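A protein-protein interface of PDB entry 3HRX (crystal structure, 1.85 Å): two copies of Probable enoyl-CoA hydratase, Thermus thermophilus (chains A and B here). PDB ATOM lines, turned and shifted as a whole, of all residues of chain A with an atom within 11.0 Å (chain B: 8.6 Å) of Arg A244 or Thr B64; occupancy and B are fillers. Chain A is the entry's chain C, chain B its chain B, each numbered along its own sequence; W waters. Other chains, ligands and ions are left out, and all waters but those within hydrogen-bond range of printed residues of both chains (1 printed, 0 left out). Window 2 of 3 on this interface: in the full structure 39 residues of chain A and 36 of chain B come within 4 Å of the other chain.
His A236 touches Phe B66.
Glu A237 touches Phe B66 (CA to CZ, 3.9999 Å).
O of Gly A239 touches CG2 of Ile B131, at 3.9 Å.
CD2 of Phe B66 touches CG1 of Val A240 (3.3 Å).
Leu B63 touches Phe A243 (CD1 to CD1, 3.9 Å).
Hydrophobic or aromatic side chains of chain B that line the printed part of chain A: Leu B63, Phe B66, Tyr B73 and Ile B131.
Among the printed residues, 10 pairs touch across the chains.
Among the printed residues, no Asp or Glu carboxylate lies within 4 Å of a Lys or Arg side-chain nitrogen of the other chain.
The backbone carbonyl oxygen (O) of Leu B63 sits at hydrogen-bond distance from the guanidinium group (NH2) of Arg A244.
The backbone carbonyl oxygen of Thr B64 lies within hydrogen-bond range of the guanidinium group of Arg A244.
The backbone carbonyl oxygen (O) of Phe B66 is in hydrogen-bond range of the guanidinium group (NH2) of Arg A244, at 2.8 Å.
The side-chain hydroxyl of Tyr B73 is in hydrogen-bond range of a ring nitrogen (NE2) of His A236 (2.6 Å).
The backbone carbonyl oxygen (O) of Ile B131 sits at hydrogen-bond distance from a ring nitrogen (ND1) of His A236, 2.8 Å away.
The side-chain carboxylate of Asp B62 sits at hydrogen-bond distance from the side-chain hydroxyl of Thr B64 (2.6 Å).
No position is printed for both chains.
Water W1 lies within hydrogen-bond range of the guanidinium group (NE) of Arg A244, the backbone carbonyl oxygen (O) of Leu B63 and the backbone NH (N) of Thr B64.
Arg A244 touches just these residues of chain B: Leu B63, Thr B64 and Phe B66.
Thr B64 touches just one residue of chain A: Arg A244.
No residue of chain A comes within 4 Å of Asp B62.
Of the printed residues of chain A, Leu B63 touches Phe A243 and Arg A244.
No residue of chain A comes within 4 Å of Glu B65.
Printed residues of chain B within 4 Å of Glu A237: Phe B66.
Printed residues of chain A within 4 Å of Tyr B73: His A236.
Printed residues of chain B within 4 Å of Val A240: Phe B66 (3.3 Å).
Printed residues of chain A within 4 Å of Ile B131: His A236 and Gly A239.
Arg B17 touches none of the printed residues of chain A.
The nearest residue of chain B that does not touch Arg A244 is Glu B65 (4.5 Å).
The nearest residue of chain A that does not touch Thr B64 is Val A240 (6.8 Å).
The nearest printed residue of chain B that does not touch Gly A239 is Leu B63 (6.1 Å).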
ATOM      1  N   ASP A 235     -22.277  -7.979 -18.594  1.00  0.00           N
ATOM      2  CA  ASP A 235     -21.726  -6.796 -17.942  1.00  0.00           C
ATOM      3  C   ASP A 235     -22.652  -5.606 -18.171  1.00  0.00           C
ATOM      4  O   ASP A 235     -22.785  -4.741 -17.307  1.00  0.00           O
ATOM      5  CB  ASP A 235     -20.326  -6.472 -18.481  1.00  0.00           C
ATOM      6  CG  ASP A 235     -19.226  -7.201 -17.727  1.00  0.00           C
ATOM      7  OD1 ASP A 235     -18.040  -7.030 -18.087  1.00  0.00           O
ATOM      8  OD2 ASP A 235     -19.545  -7.941 -16.772  1.00  0.00           O
ATOM      9  N   HIS A 236     -23.297  -5.555 -19.335  1.00  0.00           N
ATOM     10  CA  HIS A 236     -24.206  -4.452 -19.611  1.00  0.00           C
ATOM     11  C   HIS A 236     -25.437  -4.568 -18.728  1.00  0.00           C
ATOM     12  O   HIS A 236     -25.942  -3.569 -18.216  1.00  0.00           O
ATOM     13  CB  HIS A 236     -24.643  -4.431 -21.076  1.00  0.00           C
ATOM     14  CG  HIS A 236     -25.703  -3.414 -21.362  1.00  0.00           C
ATOM     15  ND1 HIS A 236     -25.583  -2.091 -20.989  1.00  0.00           N
ATOM     16  CD2 HIS A 236     -26.916  -3.527 -21.954  1.00  0.00           C
ATOM     17  CE1 HIS A 236     -26.674  -1.435 -21.338  1.00  0.00           C
ATOM     18  NE2 HIS A 236     -27.499  -2.284 -21.926  1.00  0.00           N
ATOM     19  N   GLU A 237     -25.924  -5.792 -18.556  1.00  0.00           N
ATOM     20  CA  GLU A 237     -27.096  -6.019 -17.718  1.00  0.00           C
ATOM     21  C   GLU A 237     -26.758  -5.557 -16.302  1.00  0.00           C
ATOM     22  O   GLU A 237     -27.513  -4.807 -15.683  1.00  0.00           O
ATOM     23  CB  GLU A 237     -27.466  -7.503 -17.722  1.00  0.00           C
ATOM     24  CG  GLU A 237     -28.756  -7.833 -16.990  1.00  0.00           C
ATOM     25  CD  GLU A 237     -29.125  -9.300 -17.104  1.00  0.00           C
ATOM     26  OE1 GLU A 237     -28.327 -10.151 -16.654  1.00  0.00           O
ATOM     27  OE2 GLU A 237     -30.210  -9.603 -17.645  1.00  0.00           O
ATOM     28  N   GLU A 238     -25.610  -6.006 -15.804  1.00  0.00           N
ATOM     29  CA  GLU A 238     -25.136  -5.636 -14.474  1.00  0.00           C
ATOM     30  C   GLU A 238     -24.982  -4.122 -14.397  1.00  0.00           C
ATOM     31  O   GLU A 238     -25.330  -3.496 -13.394  1.00  0.00           O
ATOM     32  CB  GLU A 238     -23.792  -6.321 -14.196  1.00  0.00           C
ATOM     33  CG  GLU A 238     -23.024  -5.795 -12.989  1.00  0.00           C
ATOM     34  CD  GLU A 238     -23.717  -6.067 -11.666  1.00  0.00           C
ATOM     35  OE1 GLU A 238     -23.159  -5.669 -10.621  1.00  0.00           O
ATOM     36  OE2 GLU A 238     -24.812  -6.673 -11.665  1.00  0.00           O
ATOM     37  N   GLY A 239     -24.461  -3.533 -15.470  1.00  0.00           N
ATOM     38  CA  GLY A 239     -24.277  -2.095 -15.499  1.00  0.00           C
ATOM     39  C   GLY A 239     -25.580  -1.351 -15.285  1.00  0.00           C
ATOM     40  O   GLY A 239     -25.655  -0.445 -14.456  1.00  0.00           O
ATOM     41  N   VAL A 240     -26.613  -1.732 -16.032  1.00  0.00           N
ATOM     42  CA  VAL A 240     -27.919  -1.089 -15.916  1.00  0.00           C
ATOM     43  C   VAL A 240     -28.527  -1.340 -14.537  1.00  0.00           C
ATOM     44  O   VAL A 240     -29.079  -0.429 -13.916  1.00  0.00           O
ATOM     45  CB  VAL A 240     -28.899  -1.607 -16.992  1.00  0.00           C
ATOM     46  CG1 VAL A 240     -30.247  -0.916 -16.846  1.00  0.00           C
ATOM     47  CG2 VAL A 240     -28.326  -1.358 -18.381  1.00  0.00           C
ATOM     48  N   ARG A 241     -28.423  -2.579 -14.063  1.00  0.00           N
ATOM     49  CA  ARG A 241     -28.961  -2.941 -12.755  1.00  0.00           C
ATOM     50  C   ARG A 241     -28.288  -2.127 -11.655  1.00  0.00           C
ATOM     51  O   ARG A 241     -28.958  -1.576 -10.781  1.00  0.00           O
ATOM     52  CB  ARG A 241     -28.762  -4.431 -12.502  1.00  0.00           C
ATOM     53  N   ALA A 242     -26.961  -2.048 -11.706  1.00  0.00           N
ATOM     54  CA  ALA A 242     -26.203  -1.300 -10.709  1.00  0.00           C
ATOM     55  C   ALA A 242     -26.594   0.176 -10.714  1.00  0.00           C
ATOM     56  O   ALA A 242     -26.625   0.819  -9.667  1.00  0.00           O
ATOM     57  CB  ALA A 242     -24.706  -1.445 -10.972  1.00  0.00           C
ATOM     58  N   PHE A 243     -26.890   0.708 -11.897  1.00  0.00           N
ATOM     59  CA  PHE A 243     -27.279   2.108 -12.021  1.00  0.00           C
ATOM     60  C   PHE A 243     -28.649   2.346 -11.394  1.00  0.00           C
ATOM     61  O   PHE A 243     -28.851   3.327 -10.679  1.00  0.00           O
ATOM     62  CB  PHE A 243     -27.295   2.526 -13.496  1.00  0.00           C
ATOM     63  CG  PHE A 243     -27.806   3.922 -13.726  1.00  0.00           C
ATOM     64  CD1 PHE A 243     -29.166   4.161 -13.907  1.00  0.00           C
ATOM     65  CD2 PHE A 243     -26.928   5.002 -13.743  1.00  0.00           C
ATOM     66  CE1 PHE A 243     -29.645   5.456 -14.100  1.00  0.00           C
ATOM     67  CE2 PHE A 243     -27.397   6.300 -13.937  1.00  0.00           C
ATOM     68  CZ  PHE A 243     -28.758   6.528 -14.115  1.00  0.00           C
ATOM     69  N   ARG A 244     -29.587   1.448 -11.670  1.00  0.00           N
ATOM     70  CA  ARG A 244     -30.931   1.559 -11.118  1.00  0.00           C
ATOM     71  C   ARG A 244     -30.875   1.383  -9.606  1.00  0.00           C
ATOM     72  O   ARG A 244     -31.458   2.164  -8.856  1.00  0.00           O
ATOM     73  CB  ARG A 244     -31.844   0.493 -11.724  1.00  0.00           C
ATOM     74  CG  ARG A 244     -32.221   0.737 -13.173  1.00  0.00           C
ATOM     75  CD  ARG A 244     -32.892  -0.489 -13.768  1.00  0.00           C
ATOM     76  NE  ARG A 244     -33.439  -0.230 -15.096  1.00  0.00           N
ATOM     77  CZ  ARG A 244     -33.915  -1.171 -15.905  1.00  0.00           C
ATOM     78  NH1 ARG A 244     -33.910  -2.443 -15.525  1.00  0.00           N
ATOM     79  NH2 ARG A 244     -34.401  -0.839 -17.094  1.00  0.00           N
ATOM     80  N   GLU A 245     -30.162   0.350  -9.170  1.00  0.00           N
ATOM     81  CA  GLU A 245     -30.023   0.049  -7.750  1.00  0.00           C
ATOM     82  C   GLU A 245     -29.089   1.025  -7.043  1.00  0.00           C
ATOM     83  O   GLU A 245     -28.836   0.896  -5.845  1.00  0.00           O
ATOM     84  CB  GLU A 245     -29.516  -1.382  -7.576  1.00  0.00           C
ATOM     85  CG  GLU A 245     -30.487  -2.436  -8.084  1.00  0.00           C
ATOM     86  CD  GLU A 245     -29.871  -3.818  -8.151  1.00  0.00           C
ATOM     87  OE1 GLU A 245     -29.283  -4.259  -7.142  1.00  0.00           O
ATOM     88  OE2 GLU A 245     -29.980  -4.467  -9.212  1.00  0.00           O
ATOM     89  N   LYS A 246     -28.585   2.002  -7.791  1.00  0.00           N
ATOM     90  CA  LYS A 246     -27.685   3.011  -7.242  1.00  0.00           C
ATOM     91  C   LYS A 246     -26.521   2.381  -6.479  1.00  0.00           C
ATOM     92  O   LYS A 246     -26.181   2.816  -5.379  1.00  0.00           O
ATOM     93  CB  LYS A 246     -28.461   3.957  -6.326  1.00  0.00           C
ATOM     94  N   ARG A 247     -25.912   1.359  -7.073  1.00  0.00           N
ATOM     95  CA  ARG A 247     -24.789   0.665  -6.453  1.00  0.00           C
ATOM     96  C   ARG A 247     -23.670   0.464  -7.467  1.00  0.00           C
ATOM     97  O   ARG A 247     -23.903   0.489  -8.674  1.00  0.00           O
ATOM     98  CB  ARG A 247     -25.236  -0.701  -5.932  1.00  0.00           C
ATOM     99  CG  ARG A 247     -25.701  -1.645  -7.028  1.00  0.00           C
ATOM    100  CD  ARG A 247     -26.074  -3.008  -6.475  1.00  0.00           C
ATOM    101  NE  ARG A 247     -26.563  -3.910  -7.517  1.00  0.00           N
ATOM    102  CZ  ARG A 247     -25.823  -4.364  -8.523  1.00  0.00           C
ATOM    103  NH1 ARG A 247     -24.550  -4.004  -8.630  1.00  0.00           N
ATOM    104  NH2 ARG A 247     -26.356  -5.178  -9.426  1.00  0.00           N
ATOM    105  N   PRO A 248     -22.433   0.262  -6.986  1.00  0.00           N
ATOM    106  CA  PRO A 248     -21.309   0.055  -7.902  1.00  0.00           C
ATOM    107  C   PRO A 248     -21.466  -1.287  -8.609  1.00  0.00           C
ATOM    108  O   PRO A 248     -21.801  -2.294  -7.983  1.00  0.00           O
ATOM    109  CB  PRO A 248     -20.103   0.087  -6.971  1.00  0.00           C
ATOM    110  CG  PRO A 248     -20.650  -0.514  -5.714  1.00  0.00           C
ATOM    111  CD  PRO A 248     -21.987   0.183  -5.585  1.00  0.00           C
ATOM    112  N   PRO A 249     -21.234  -1.319  -9.928  1.00  0.00           N
ATOM    113  CA  PRO A 249     -21.362  -2.566 -10.685  1.00  0.00           C
ATOM    114  C   PRO A 249     -20.205  -3.530 -10.437  1.00  0.00           C
ATOM    115  O   PRO A 249     -19.102  -3.113 -10.085  1.00  0.00           O
ATOM    116  CB  PRO A 249     -21.410  -2.078 -12.128  1.00  0.00           C
ATOM    117  CG  PRO A 249     -20.481  -0.902 -12.092  1.00  0.00           C
ATOM    118  CD  PRO A 249     -20.897  -0.193 -10.819  1.00  0.00           C
ATOM    119  N   PHE A 251     -18.403  -5.930 -12.619  1.00  0.00           N
ATOM    120  CA  PHE A 251     -18.134  -6.436 -13.961  1.00  0.00           C
ATOM    121  C   PHE A 251     -17.256  -7.684 -13.982  1.00  0.00           C
ATOM    122  O   PHE A 251     -16.394  -7.863 -13.123  1.00  0.00           O
ATOM    123  CB  PHE A 251     -17.490  -5.328 -14.800  1.00  0.00           C
ATOM    124  CG  PHE A 251     -18.379  -4.130 -15.009  1.00  0.00           C
ATOM    125  CD1 PHE A 251     -17.943  -2.854 -14.661  1.00  0.00           C
ATOM    126  CD2 PHE A 251     -19.648  -4.275 -15.566  1.00  0.00           C
ATOM    127  CE1 PHE A 251     -18.755  -1.738 -14.866  1.00  0.00           C
ATOM    128  CE2 PHE A 251     -20.470  -3.165 -15.775  1.00  0.00           C
ATOM    129  CZ  PHE A 251     -20.021  -1.895 -15.424  1.00  0.00           C
ATOM    130  N   ARG B  17     -37.833  17.491 -21.789  1.00  0.00           N
ATOM    131  CA  ARG B  17     -38.202  16.429 -20.855  1.00  0.00           C
ATOM    132  C   ARG B  17     -37.364  16.735 -19.617  1.00  0.00           C
ATOM    133  O   ARG B  17     -36.664  15.868 -19.098  1.00  0.00           O
ATOM    134  CB  ARG B  17     -37.824  15.047 -21.387  1.00  0.00           C
ATOM    135  CG  ARG B  17     -38.424  14.674 -22.725  1.00  0.00           C
ATOM    136  CD  ARG B  17     -38.095  13.229 -23.053  1.00  0.00           C
ATOM    137  NE  ARG B  17     -38.844  12.304 -22.207  1.00  0.00           N
ATOM    138  CZ  ARG B  17     -38.443  11.073 -21.906  1.00  0.00           C
ATOM    139  NH1 ARG B  17     -37.293  10.616 -22.377  1.00  0.00           N
ATOM    140  NH2 ARG B  17     -39.199  10.295 -21.141  1.00  0.00           N
ATOM    141  N   LYS B  20     -36.977  14.527 -16.565  1.00  0.00           N
ATOM    142  CA  LYS B  20     -36.159  13.337 -16.769  1.00  0.00           C
ATOM    143  C   LYS B  20     -34.777  13.712 -17.299  1.00  0.00           C
ATOM    144  O   LYS B  20     -34.097  12.895 -17.920  1.00  0.00           O
ATOM    145  CB  LYS B  20     -36.845  12.382 -17.748  1.00  0.00           C
ATOM    146  CG  LYS B  20     -38.137  11.778 -17.220  1.00  0.00           C
ATOM    147  CD  LYS B  20     -38.754  10.837 -18.240  1.00  0.00           C
ATOM    148  CE  LYS B  20     -40.013  10.179 -17.698  1.00  0.00           C
ATOM    149  NZ  LYS B  20     -39.722   9.334 -16.509  1.00  0.00           N
ATOM    150  N   ALA B  23     -33.759  12.865 -20.887  1.00  0.00           N
ATOM    151  CA  ALA B  23     -33.277  11.538 -21.232  1.00  0.00           C
ATOM    152  C   ALA B  23     -33.705  11.259 -22.665  1.00  0.00           C
ATOM    153  O   ALA B  23     -34.787  11.669 -23.094  1.00  0.00           O
ATOM    154  CB  ALA B  23     -33.870  10.495 -20.290  1.00  0.00           C
ATOM    155  N   ILE B  24     -32.854  10.555 -23.401  1.00  0.00           N
ATOM    156  CA  ILE B  24     -33.132  10.251 -24.794  1.00  0.00           C
ATOM    157  C   ILE B  24     -33.947   8.980 -25.018  1.00  0.00           C
ATOM    158  O   ILE B  24     -33.581   7.898 -24.561  1.00  0.00           O
ATOM    159  CB  ILE B  24     -31.815  10.155 -25.587  1.00  0.00           C
ATOM    160  CG1 ILE B  24     -31.067  11.489 -25.491  1.00  0.00           C
ATOM    161  CG2 ILE B  24     -32.101   9.787 -27.034  1.00  0.00           C
ATOM    162  CD1 ILE B  24     -29.747  11.517 -26.218  1.00  0.00           C
ATOM    163  N   THR B  25     -35.057   9.130 -25.732  1.00  0.00           N
ATOM    164  CA  THR B  25     -35.932   8.010 -26.054  1.00  0.00           C
ATOM    165  C   THR B  25     -36.189   8.023 -27.549  1.00  0.00           C
ATOM    166  O   THR B  25     -35.872   8.999 -28.234  1.00  0.00           O
ATOM    167  CB  THR B  25     -37.293   8.122 -25.345  1.00  0.00           C
ATOM    168  OG1 THR B  25     -37.948   9.330 -25.757  1.00  0.00           O
ATOM    169  CG2 THR B  25     -37.110   8.122 -23.837  1.00  0.00           C
ATOM    170  N   GLN B  61     -29.280   8.273 -22.958  1.00  0.00           N
ATOM    171  CA  GLN B  61     -30.328   7.280 -23.167  1.00  0.00           C
ATOM    172  C   GLN B  61     -31.135   6.973 -21.910  1.00  0.00           C
ATOM    173  O   GLN B  61     -30.575   6.713 -20.844  1.00  0.00           O
ATOM    174  CB  GLN B  61     -29.715   5.982 -23.702  1.00  0.00           C
ATOM    175  CG  GLN B  61     -30.694   4.817 -23.832  1.00  0.00           C
ATOM    176  CD  GLN B  61     -31.805   5.080 -24.834  1.00  0.00           C
ATOM    177  OE1 GLN B  61     -31.549   5.377 -26.001  1.00  0.00           O
ATOM    178  NE2 GLN B  61     -33.049   4.964 -24.382  1.00  0.00           N
ATOM    179  N   ASP B  62     -32.456   7.012 -22.046  1.00  0.00           N
ATOM    180  CA  ASP B  62     -33.355   6.707 -20.939  1.00  0.00           C
ATOM    181  C   ASP B  62     -33.342   5.183 -20.803  1.00  0.00           C
ATOM    182  O   ASP B  62     -33.656   4.469 -21.758  1.00  0.00           O
ATOM    183  CB  ASP B  62     -34.768   7.200 -21.262  1.00  0.00           C
ATOM    184  CG  ASP B  62     -35.723   7.028 -20.101  1.00  0.00           C
ATOM    185  OD1 ASP B  62     -35.827   5.897 -19.586  1.00  0.00           O
ATOM    186  OD2 ASP B  62     -36.371   8.021 -19.706  1.00  0.00           O
ATOM    187  N   LEU B  63     -32.981   4.691 -19.623  1.00  0.00           N
ATOM    188  CA  LEU B  63     -32.888   3.251 -19.388  1.00  0.00           C
ATOM    189  C   LEU B  63     -34.156   2.563 -18.881  1.00  0.00           C
ATOM    190  O   LEU B  63     -34.133   1.366 -18.596  1.00  0.00           O
ATOM    191  CB  LEU B  63     -31.746   2.966 -18.407  1.00  0.00           C
ATOM    192  CG  LEU B  63     -30.352   3.476 -18.786  1.00  0.00           C
ATOM    193  CD1 LEU B  63     -29.374   3.160 -17.669  1.00  0.00           C
ATOM    194  CD2 LEU B  63     -29.901   2.834 -20.090  1.00  0.00           C
ATOM    195  N   THR B  64     -35.257   3.301 -18.780  1.00  0.00           N
ATOM    196  CA  THR B  64     -36.508   2.731 -18.282  1.00  0.00           C
ATOM    197  C   THR B  64     -36.972   1.449 -18.973  1.00  0.00           C
ATOM    198  O   THR B  64     -37.370   0.494 -18.307  1.00  0.00           O
ATOM    199  CB  THR B  64     -37.662   3.749 -18.358  1.00  0.00           C
ATOM    200  OG1 THR B  64     -37.793   4.224 -19.703  1.00  0.00           O
ATOM    201  CG2 THR B  64     -37.407   4.920 -17.420  1.00  0.00           C
ATOM    202  N   GLU B  65     -36.922   1.419 -20.301  1.00  0.00           N
ATOM    203  CA  GLU B  65     -37.373   0.246 -21.046  1.00  0.00           C
ATOM    204  C   GLU B  65     -36.438  -0.963 -21.050  1.00  0.00           C
ATOM    205  O   GLU B  65     -36.772  -1.997 -21.629  1.00  0.00           O
ATOM    206  CB  GLU B  65     -37.695   0.629 -22.493  1.00  0.00           C
ATOM    207  CG  GLU B  65     -38.912   1.527 -22.638  1.00  0.00           C
ATOM    208  CD  GLU B  65     -39.353   1.680 -24.080  1.00  0.00           C
ATOM    209  OE1 GLU B  65     -38.544   2.149 -24.909  1.00  0.00           O
ATOM    210  OE2 GLU B  65     -40.512   1.330 -24.388  1.00  0.00           O
ATOM    211  N   PHE B  66     -35.278  -0.850 -20.409  1.00  0.00           N
ATOM    212  CA  PHE B  66     -34.344  -1.974 -20.380  1.00  0.00           C
ATOM    213  C   PHE B  66     -34.924  -3.137 -19.579  1.00  0.00           C
ATOM    214  O   PHE B  66     -35.547  -2.937 -18.536  1.00  0.00           O
ATOM    215  CB  PHE B  66     -33.003  -1.560 -19.767  1.00  0.00           C
ATOM    216  CG  PHE B  66     -31.936  -2.619 -19.879  1.00  0.00           C
ATOM    217  CD1 PHE B  66     -31.360  -2.917 -21.111  1.00  0.00           C
ATOM    218  CD2 PHE B  66     -31.527  -3.337 -18.759  1.00  0.00           C
ATOM    219  CE1 PHE B  66     -30.391  -3.915 -21.228  1.00  0.00           C
ATOM    220  CE2 PHE B  66     -30.558  -4.338 -18.864  1.00  0.00           C
ATOM    221  CZ  PHE B  66     -29.990  -4.626 -20.102  1.00  0.00           C
ATOM    222  N   GLY B  67     -34.712  -4.353 -20.075  1.00  0.00           N
ATOM    223  CA  GLY B  67     -35.221  -5.530 -19.395  1.00  0.00           C
ATOM    224  C   GLY B  67     -36.545  -5.988 -19.972  1.00  0.00           C
ATOM    225  O   GLY B  67     -36.925  -7.151 -19.835  1.00  0.00           O
ATOM    226  N   ASP B  68     -37.248  -5.067 -20.623  1.00  0.00           N
ATOM    227  CA  ASP B  68     -38.540  -5.361 -21.232  1.00  0.00           C
ATOM    228  C   ASP B  68     -38.424  -6.434 -22.311  1.00  0.00           C
ATOM    229  O   ASP B  68     -39.402  -7.107 -22.633  1.00  0.00           O
ATOM    230  CB  ASP B  68     -39.137  -4.086 -21.834  1.00  0.00           C
ATOM    231  CG  ASP B  68     -39.548  -3.079 -20.776  1.00  0.00           C
ATOM    232  OD1 ASP B  68     -38.730  -2.787 -19.878  1.00  0.00           O
ATOM    233  OD2 ASP B  68     -40.689  -2.575 -20.845  1.00  0.00           O
ATOM    234  N   ARG B  69     -37.225  -6.589 -22.865  1.00  0.00           N
ATOM    235  CA  ARG B  69     -36.987  -7.581 -23.909  1.00  0.00           C
ATOM    236  C   ARG B  69     -35.498  -7.720 -24.207  1.00  0.00           C
ATOM    237  O   ARG B  69     -34.671  -7.017 -23.626  1.00  0.00           O
ATOM    238  CB  ARG B  69     -37.736  -7.191 -25.180  1.00  0.00           C
ATOM    239  N   TYR B  73     -29.458  -3.369 -29.489  1.00  0.00           N
ATOM    240  CA  TYR B  73     -28.887  -2.055 -29.757  1.00  0.00           C
ATOM    241  C   TYR B  73     -28.529  -1.817 -31.215  1.00  0.00           C
ATOM    242  O   TYR B  73     -28.536  -0.675 -31.670  1.00  0.00           O
ATOM    243  CB  TYR B  73     -27.654  -1.808 -28.884  1.00  0.00           C
ATOM    244  CG  TYR B  73     -27.981  -1.567 -27.428  1.00  0.00           C
ATOM    245  CD1 TYR B  73     -28.277  -2.627 -26.575  1.00  0.00           C
ATOM    246  CD2 TYR B  73     -28.036  -0.271 -26.913  1.00  0.00           C
ATOM    247  CE1 TYR B  73     -28.620  -2.408 -25.246  1.00  0.00           C
ATOM    248  CE2 TYR B  73     -28.380  -0.039 -25.583  1.00  0.00           C
ATOM    249  CZ  TYR B  73     -28.672  -1.113 -24.757  1.00  0.00           C
ATOM    250  OH  TYR B  73     -29.028  -0.895 -23.446  1.00  0.00           O
ATOM    251  N   ILE B 131     -21.791   1.675 -17.974  1.00  0.00           N
ATOM    252  CA  ILE B 131     -22.824   0.642 -18.016  1.00  0.00           C
ATOM    253  C   ILE B 131     -22.453  -0.452 -19.021  1.00  0.00           C
ATOM    254  O   ILE B 131     -23.319  -1.143 -19.565  1.00  0.00           O
ATOM    255  CB  ILE B 131     -24.220   1.221 -18.356  1.00  0.00           C
ATOM    256  CG1 ILE B 131     -24.167   2.018 -19.658  1.00  0.00           C
ATOM    257  CG2 ILE B 131     -24.711   2.097 -17.205  1.00  0.00           C
ATOM    258  CD1 ILE B 131     -25.515   2.569 -20.080  1.00  0.00           C
HETATM  259  O   HOH W   1     -33.986   2.432 -15.855  1.00  0.00           O
